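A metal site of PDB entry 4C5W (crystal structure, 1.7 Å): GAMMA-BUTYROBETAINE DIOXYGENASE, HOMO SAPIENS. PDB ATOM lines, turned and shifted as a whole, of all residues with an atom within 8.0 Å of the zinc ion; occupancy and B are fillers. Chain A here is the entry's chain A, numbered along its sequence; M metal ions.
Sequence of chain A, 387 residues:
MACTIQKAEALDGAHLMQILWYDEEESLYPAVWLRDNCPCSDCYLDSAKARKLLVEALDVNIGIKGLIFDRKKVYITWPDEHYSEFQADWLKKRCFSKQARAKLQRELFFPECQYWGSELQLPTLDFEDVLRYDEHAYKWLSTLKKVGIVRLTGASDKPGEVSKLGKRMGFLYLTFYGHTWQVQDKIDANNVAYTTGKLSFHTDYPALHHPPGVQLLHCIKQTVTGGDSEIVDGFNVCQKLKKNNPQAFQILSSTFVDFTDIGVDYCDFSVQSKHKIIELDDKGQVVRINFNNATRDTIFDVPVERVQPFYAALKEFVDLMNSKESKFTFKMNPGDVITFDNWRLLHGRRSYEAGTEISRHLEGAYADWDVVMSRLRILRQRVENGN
The zinc ion is bound by NE2 of His 82, 2.1 Å away.
The zinc ion is bound by the side-chain sulfur (SG) of Cys 40 (2.3 Å).
The side-chain sulfur (SG) of Cys 43 binds the zinc ion (2.3 Å).
SG of Cys 38 binds the zinc ion, at 2.3 Å.
The side-chain sulfur of Cys 40 lies close to the backbone NH of Asp 42, at 3.3 Å.
The guanidinium group (NH1) of Arg 35 lies close to the side-chain sulfur (SG) of Cys 43 (3.4 Å).
The backbone carbonyl oxygen (O) of Cys 43 is in hydrogen-bond range of the backbone NH (N) of Leu 53 (3.1 Å).
SG of Cys 38 sits close to OG of Ser 84, 3.0 Å away.
Of the 18 residues printed, 4 come within 4 Å of the zinc ion.
The nearest printed residue that does not touch the zinc ion is Arg 35 (4.1 Å).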
ATOM      1  N   LEU A  34      25.833 -19.325 -28.448  1.00  0.00           N
ATOM      2  CA  LEU A  34      25.579 -18.033 -27.828  1.00  0.00           C
ATOM      3  C   LEU A  34      25.911 -16.880 -28.787  1.00  0.00           C
ATOM      4  O   LEU A  34      25.090 -15.983 -28.978  1.00  0.00           O
ATOM      5  CB  LEU A  34      26.380 -17.918 -26.528  1.00  0.00           C
ATOM      6  CG  LEU A  34      25.907 -18.852 -25.413  1.00  0.00           C
ATOM      7  CD1 LEU A  34      26.981 -18.847 -24.321  1.00  0.00           C
ATOM      8  CD2 LEU A  34      24.568 -18.415 -24.859  1.00  0.00           C
ATOM      9  N   ARG A  35      27.072 -16.920 -29.413  1.00  0.00           N
ATOM     10  CA  ARG A  35      27.479 -15.852 -30.300  1.00  0.00           C
ATOM     11  C   ARG A  35      26.470 -15.732 -31.461  1.00  0.00           C
ATOM     12  O   ARG A  35      26.019 -14.635 -31.790  1.00  0.00           O
ATOM     13  CB  ARG A  35      28.888 -16.036 -30.845  1.00  0.00           C
ATOM     14  CG  ARG A  35      29.366 -14.942 -31.781  1.00  0.00           C
ATOM     15  CD  ARG A  35      29.375 -13.554 -31.085  1.00  0.00           C
ATOM     16  NE  ARG A  35      29.636 -12.443 -31.989  1.00  0.00           N
ATOM     17  CZ  ARG A  35      28.693 -11.783 -32.653  1.00  0.00           C
ATOM     18  NH1 ARG A  35      27.443 -12.153 -32.555  1.00  0.00           N
ATOM     19  NH2 ARG A  35      29.025 -10.767 -33.433  1.00  0.00           N
ATOM     20  N   ASP A  36      26.139 -16.893 -32.040  1.00  0.00           N
ATOM     21  CA  ASP A  36      25.156 -17.001 -33.160  1.00  0.00           C
ATOM     22  C   ASP A  36      23.808 -16.417 -32.801  1.00  0.00           C
ATOM     23  O   ASP A  36      23.090 -15.904 -33.652  1.00  0.00           O
ATOM     24  CB  ASP A  36      24.989 -18.498 -33.529  1.00  0.00           C
ATOM     25  CG  ASP A  36      24.016 -18.707 -34.652  1.00  0.00           C
ATOM     26  OD1 ASP A  36      24.213 -18.064 -35.683  1.00  0.00           O
ATOM     27  OD2 ASP A  36      23.073 -19.498 -34.480  1.00  0.00           O
ATOM     28  N   ASN A  37      23.485 -16.452 -31.504  1.00  0.00           N
ATOM     29  CA  ASN A  37      22.174 -16.046 -31.023  1.00  0.00           C
ATOM     30  C   ASN A  37      22.183 -14.779 -30.155  1.00  0.00           C
ATOM     31  O   ASN A  37      21.209 -14.484 -29.468  1.00  0.00           O
ATOM     32  CB  ASN A  37      21.492 -17.239 -30.382  1.00  0.00           C
ATOM     33  CG  ASN A  37      21.062 -18.257 -31.432  1.00  0.00           C
ATOM     34  OD1 ASN A  37      20.312 -17.903 -32.341  1.00  0.00           O
ATOM     35  ND2 ASN A  37      21.608 -19.445 -31.377  1.00  0.00           N
ATOM     36  N   CYS A  38      23.226 -13.980 -30.332  1.00  0.00           N
ATOM     37  CA  CYS A  38      23.272 -12.649 -29.696  1.00  0.00           C
ATOM     38  C   CYS A  38      21.998 -11.889 -30.040  1.00  0.00           C
ATOM     39  O   CYS A  38      21.629 -11.798 -31.200  1.00  0.00           O
ATOM     40  CB  CYS A  38      24.493 -11.883 -30.183  1.00  0.00           C
ATOM     41  SG  CYS A  38      24.549 -10.232 -29.409  1.00  0.00           S
ATOM     42  N   PRO A  39      21.295 -11.358 -29.042  1.00  0.00           N
ATOM     43  CA  PRO A  39      20.042 -10.636 -29.346  1.00  0.00           C
ATOM     44  C   PRO A  39      20.193  -9.133 -29.555  1.00  0.00           C
ATOM     45  O   PRO A  39      19.186  -8.419 -29.583  1.00  0.00           O
ATOM     46  CB  PRO A  39      19.184 -10.926 -28.119  1.00  0.00           C
ATOM     47  CG  PRO A  39      20.175 -11.054 -27.019  1.00  0.00           C
ATOM     48  CD  PRO A  39      21.388 -11.711 -27.618  1.00  0.00           C
ATOM     49  N   CYS A  40      21.422  -8.634 -29.674  1.00  0.00           N
ATOM     50  CA  CYS A  40      21.620  -7.199 -29.812  1.00  0.00           C
ATOM     51  C   CYS A  40      21.134  -6.734 -31.172  1.00  0.00           C
ATOM     52  O   CYS A  40      20.925  -7.534 -32.092  1.00  0.00           O
ATOM     53  CB  CYS A  40      23.104  -6.823 -29.630  1.00  0.00           C
ATOM     54  SG  CYS A  40      24.133  -6.906 -31.123  1.00  0.00           S
ATOM     55  N   SER A  41      20.976  -5.425 -31.334  1.00  0.00           N
ATOM     56  CA  SER A  41      20.359  -4.919 -32.558  1.00  0.00           C
ATOM     57  C   SER A  41      21.263  -5.088 -33.786  1.00  0.00           C
ATOM     58  O   SER A  41      20.771  -5.054 -34.935  1.00  0.00           O
ATOM     59  CB  SER A  41      19.974  -3.447 -32.395  1.00  0.00           C
ATOM     60  OG  SER A  41      21.126  -2.682 -32.111  1.00  0.00           O
ATOM     61  N   ASP A  42      22.584  -5.253 -33.585  1.00  0.00           N
ATOM     62  CA  ASP A  42      23.441  -5.609 -34.720  1.00  0.00           C
ATOM     63  C   ASP A  42      23.148  -7.025 -35.235  1.00  0.00           C
ATOM     64  O   ASP A  42      23.290  -7.270 -36.434  1.00  0.00           O
ATOM     65  CB  ASP A  42      24.934  -5.622 -34.404  1.00  0.00           C
ATOM     66  CG  ASP A  42      25.514  -4.258 -34.076  1.00  0.00           C
ATOM     67  OD1 ASP A  42      24.830  -3.230 -34.253  1.00  0.00           O
ATOM     68  OD2 ASP A  42      26.720  -4.233 -33.762  1.00  0.00           O
ATOM     69  N   CYS A  43      22.820  -7.941 -34.341  1.00  0.00           N
ATOM     70  CA  CYS A  43      22.765  -9.354 -34.670  1.00  0.00           C
ATOM     71  C   CYS A  43      21.375  -9.850 -34.937  1.00  0.00           C
ATOM     72  O   CYS A  43      21.217 -10.920 -35.497  1.00  0.00           O
ATOM     73  CB  CYS A  43      23.395 -10.175 -33.537  1.00  0.00           C
ATOM     74  SG  CYS A  43      25.149  -9.818 -33.294  1.00  0.00           S
ATOM     75  N   TYR A  44      20.369  -9.080 -34.559  1.00  0.00           N
ATOM     76  CA  TYR A  44      19.031  -9.606 -34.436  1.00  0.00           C
ATOM     77  C   TYR A  44      18.044  -8.492 -34.675  1.00  0.00           C
ATOM     78  O   TYR A  44      18.112  -7.427 -34.016  1.00  0.00           O
ATOM     79  CB  TYR A  44      18.835 -10.191 -33.039  1.00  0.00           C
ATOM     80  CG  TYR A  44      17.582 -10.994 -32.866  1.00  0.00           C
ATOM     81  CD1 TYR A  44      17.552 -12.330 -33.267  1.00  0.00           C
ATOM     82  CD2 TYR A  44      16.424 -10.445 -32.331  1.00  0.00           C
ATOM     83  CE1 TYR A  44      16.419 -13.088 -33.116  1.00  0.00           C
ATOM     84  CE2 TYR A  44      15.261 -11.200 -32.184  1.00  0.00           C
ATOM     85  CZ  TYR A  44      15.276 -12.525 -32.581  1.00  0.00           C
ATOM     86  OH  TYR A  44      14.156 -13.328 -32.463  1.00  0.00           O
ATOM     87  N   LEU A  53      22.642 -11.639 -38.141  1.00  0.00           N
ATOM     88  CA  LEU A  53      24.018 -12.105 -38.158  1.00  0.00           C
ATOM     89  C   LEU A  53      24.206 -13.125 -39.291  1.00  0.00           C
ATOM     90  O   LEU A  53      23.368 -14.003 -39.458  1.00  0.00           O
ATOM     91  CB  LEU A  53      24.369 -12.749 -36.822  1.00  0.00           C
ATOM     92  CG  LEU A  53      25.811 -13.200 -36.610  1.00  0.00           C
ATOM     93  CD1 LEU A  53      26.688 -11.960 -36.394  1.00  0.00           C
ATOM     94  CD2 LEU A  53      25.896 -14.161 -35.437  1.00  0.00           C
ATOM     95  N   TRP A  78      33.139 -10.847 -26.104  1.00  0.00           N
ATOM     96  CA  TRP A  78      33.738 -11.743 -27.077  1.00  0.00           C
ATOM     97  C   TRP A  78      35.159 -11.308 -27.463  1.00  0.00           C
ATOM     98  O   TRP A  78      35.540 -10.156 -27.300  1.00  0.00           O
ATOM     99  CB  TRP A  78      32.827 -11.855 -28.315  1.00  0.00           C
ATOM    100  CG  TRP A  78      31.463 -12.413 -28.018  1.00  0.00           C
ATOM    101  CD1 TRP A  78      30.286 -11.734 -27.991  1.00  0.00           C
ATOM    102  CD2 TRP A  78      31.143 -13.757 -27.672  1.00  0.00           C
ATOM    103  NE1 TRP A  78      29.255 -12.563 -27.667  1.00  0.00           N
ATOM    104  CE2 TRP A  78      29.748 -13.813 -27.460  1.00  0.00           C
ATOM    105  CE3 TRP A  78      31.904 -14.917 -27.516  1.00  0.00           C
ATOM    106  CZ2 TRP A  78      29.098 -14.996 -27.103  1.00  0.00           C
ATOM    107  CZ3 TRP A  78      31.245 -16.105 -27.169  1.00  0.00           C
ATOM    108  CH2 TRP A  78      29.864 -16.131 -26.963  1.00  0.00           C
ATOM    109  N   HIS A  82      32.947  -7.764 -29.425  1.00  0.00           N
ATOM    110  CA  HIS A  82      31.485  -7.759 -29.458  1.00  0.00           C
ATOM    111  C   HIS A  82      30.958  -8.061 -28.045  1.00  0.00           C
ATOM    112  O   HIS A  82      31.646  -8.735 -27.243  1.00  0.00           O
ATOM    113  CB  HIS A  82      30.960  -8.773 -30.521  1.00  0.00           C
ATOM    114  CG  HIS A  82      29.532  -8.548 -30.877  1.00  0.00           C
ATOM    115  ND1 HIS A  82      29.146  -7.551 -31.749  1.00  0.00           N
ATOM    116  CD2 HIS A  82      28.395  -9.138 -30.441  1.00  0.00           C
ATOM    117  CE1 HIS A  82      27.825  -7.553 -31.840  1.00  0.00           C
ATOM    118  NE2 HIS A  82      27.350  -8.483 -31.036  1.00  0.00           N
ATOM    119  N   TYR A  83      29.777  -7.560 -27.734  1.00  0.00           N
ATOM    120  CA  TYR A  83      29.197  -7.681 -26.408  1.00  0.00           C
ATOM    121  C   TYR A  83      27.779  -8.207 -26.478  1.00  0.00           C
ATOM    122  O   TYR A  83      27.002  -7.749 -27.319  1.00  0.00           O
ATOM    123  CB  TYR A  83      29.195  -6.296 -25.731  1.00  0.00           C
ATOM    124  CG  TYR A  83      28.393  -6.227 -24.480  1.00  0.00           C
ATOM    125  CD1 TYR A  83      28.855  -6.845 -23.324  1.00  0.00           C
ATOM    126  CD2 TYR A  83      27.178  -5.536 -24.423  1.00  0.00           C
ATOM    127  CE1 TYR A  83      28.126  -6.827 -22.169  1.00  0.00           C
ATOM    128  CE2 TYR A  83      26.445  -5.499 -23.254  1.00  0.00           C
ATOM    129  CZ  TYR A  83      26.931  -6.143 -22.118  1.00  0.00           C
ATOM    130  OH  TYR A  83      26.247  -6.132 -20.911  1.00  0.00           O
ATOM    131  N   SER A  84      27.449  -9.166 -25.623  1.00  0.00           N
ATOM    132  CA  SER A  84      26.132  -9.806 -25.632  1.00  0.00           C
ATOM    133  C   SER A  84      25.486  -9.914 -24.239  1.00  0.00           C
ATOM    134  O   SER A  84      26.176 -10.184 -23.249  1.00  0.00           O
ATOM    135  CB  SER A  84      26.234 -11.213 -26.269  1.00  0.00           C
ATOM    136  OG  SER A  84      26.778 -11.157 -27.582  1.00  0.00           O
ATOM    137  N   GLU A  85      24.153  -9.797 -24.189  1.00  0.00           N
ATOM    138  CA  GLU A  85      23.361 -10.042 -22.964  1.00  0.00           C
ATOM    139  C   GLU A  85      22.312 -11.103 -23.215  1.00  0.00           C
ATOM    140  O   GLU A  85      21.590 -11.022 -24.218  1.00  0.00           O
ATOM    141  CB  GLU A  85      22.664  -8.761 -22.473  1.00  0.00           C
ATOM    142  CG  GLU A  85      23.619  -7.638 -22.130  1.00  0.00           C
ATOM    143  CD  GLU A  85      22.943  -6.397 -21.558  1.00  0.00           C
ATOM    144  OE1 GLU A  85      21.694  -6.346 -21.506  1.00  0.00           O
ATOM    145  OE2 GLU A  85      23.710  -5.471 -21.170  1.00  0.00           O
ATOM    146  N   PHE A  86      22.228 -12.083 -22.316  1.00  0.00           N
ATOM    147  CA  PHE A  86      21.250 -13.164 -22.417  1.00  0.00           C
ATOM    148  C   PHE A  86      20.441 -13.254 -21.126  1.00  0.00           C
ATOM    149  O   PHE A  86      21.031 -13.247 -20.038  1.00  0.00           O
ATOM    150  CB  PHE A  86      21.958 -14.504 -22.611  1.00  0.00           C
ATOM    151  CG  PHE A  86      22.820 -14.550 -23.858  1.00  0.00           C
ATOM    152  CD1 PHE A  86      22.234 -14.863 -25.084  1.00  0.00           C
ATOM    153  CD2 PHE A  86      24.161 -14.300 -23.791  1.00  0.00           C
ATOM    154  CE1 PHE A  86      23.027 -14.892 -26.242  1.00  0.00           C
ATOM    155  CE2 PHE A  86      24.963 -14.338 -24.942  1.00  0.00           C
ATOM    156  CZ  PHE A  86      24.386 -14.631 -26.165  1.00  0.00           C
HETATM  157 ZN    ZN M   1      25.268  -8.908 -31.171  1.00  0.00          ZN
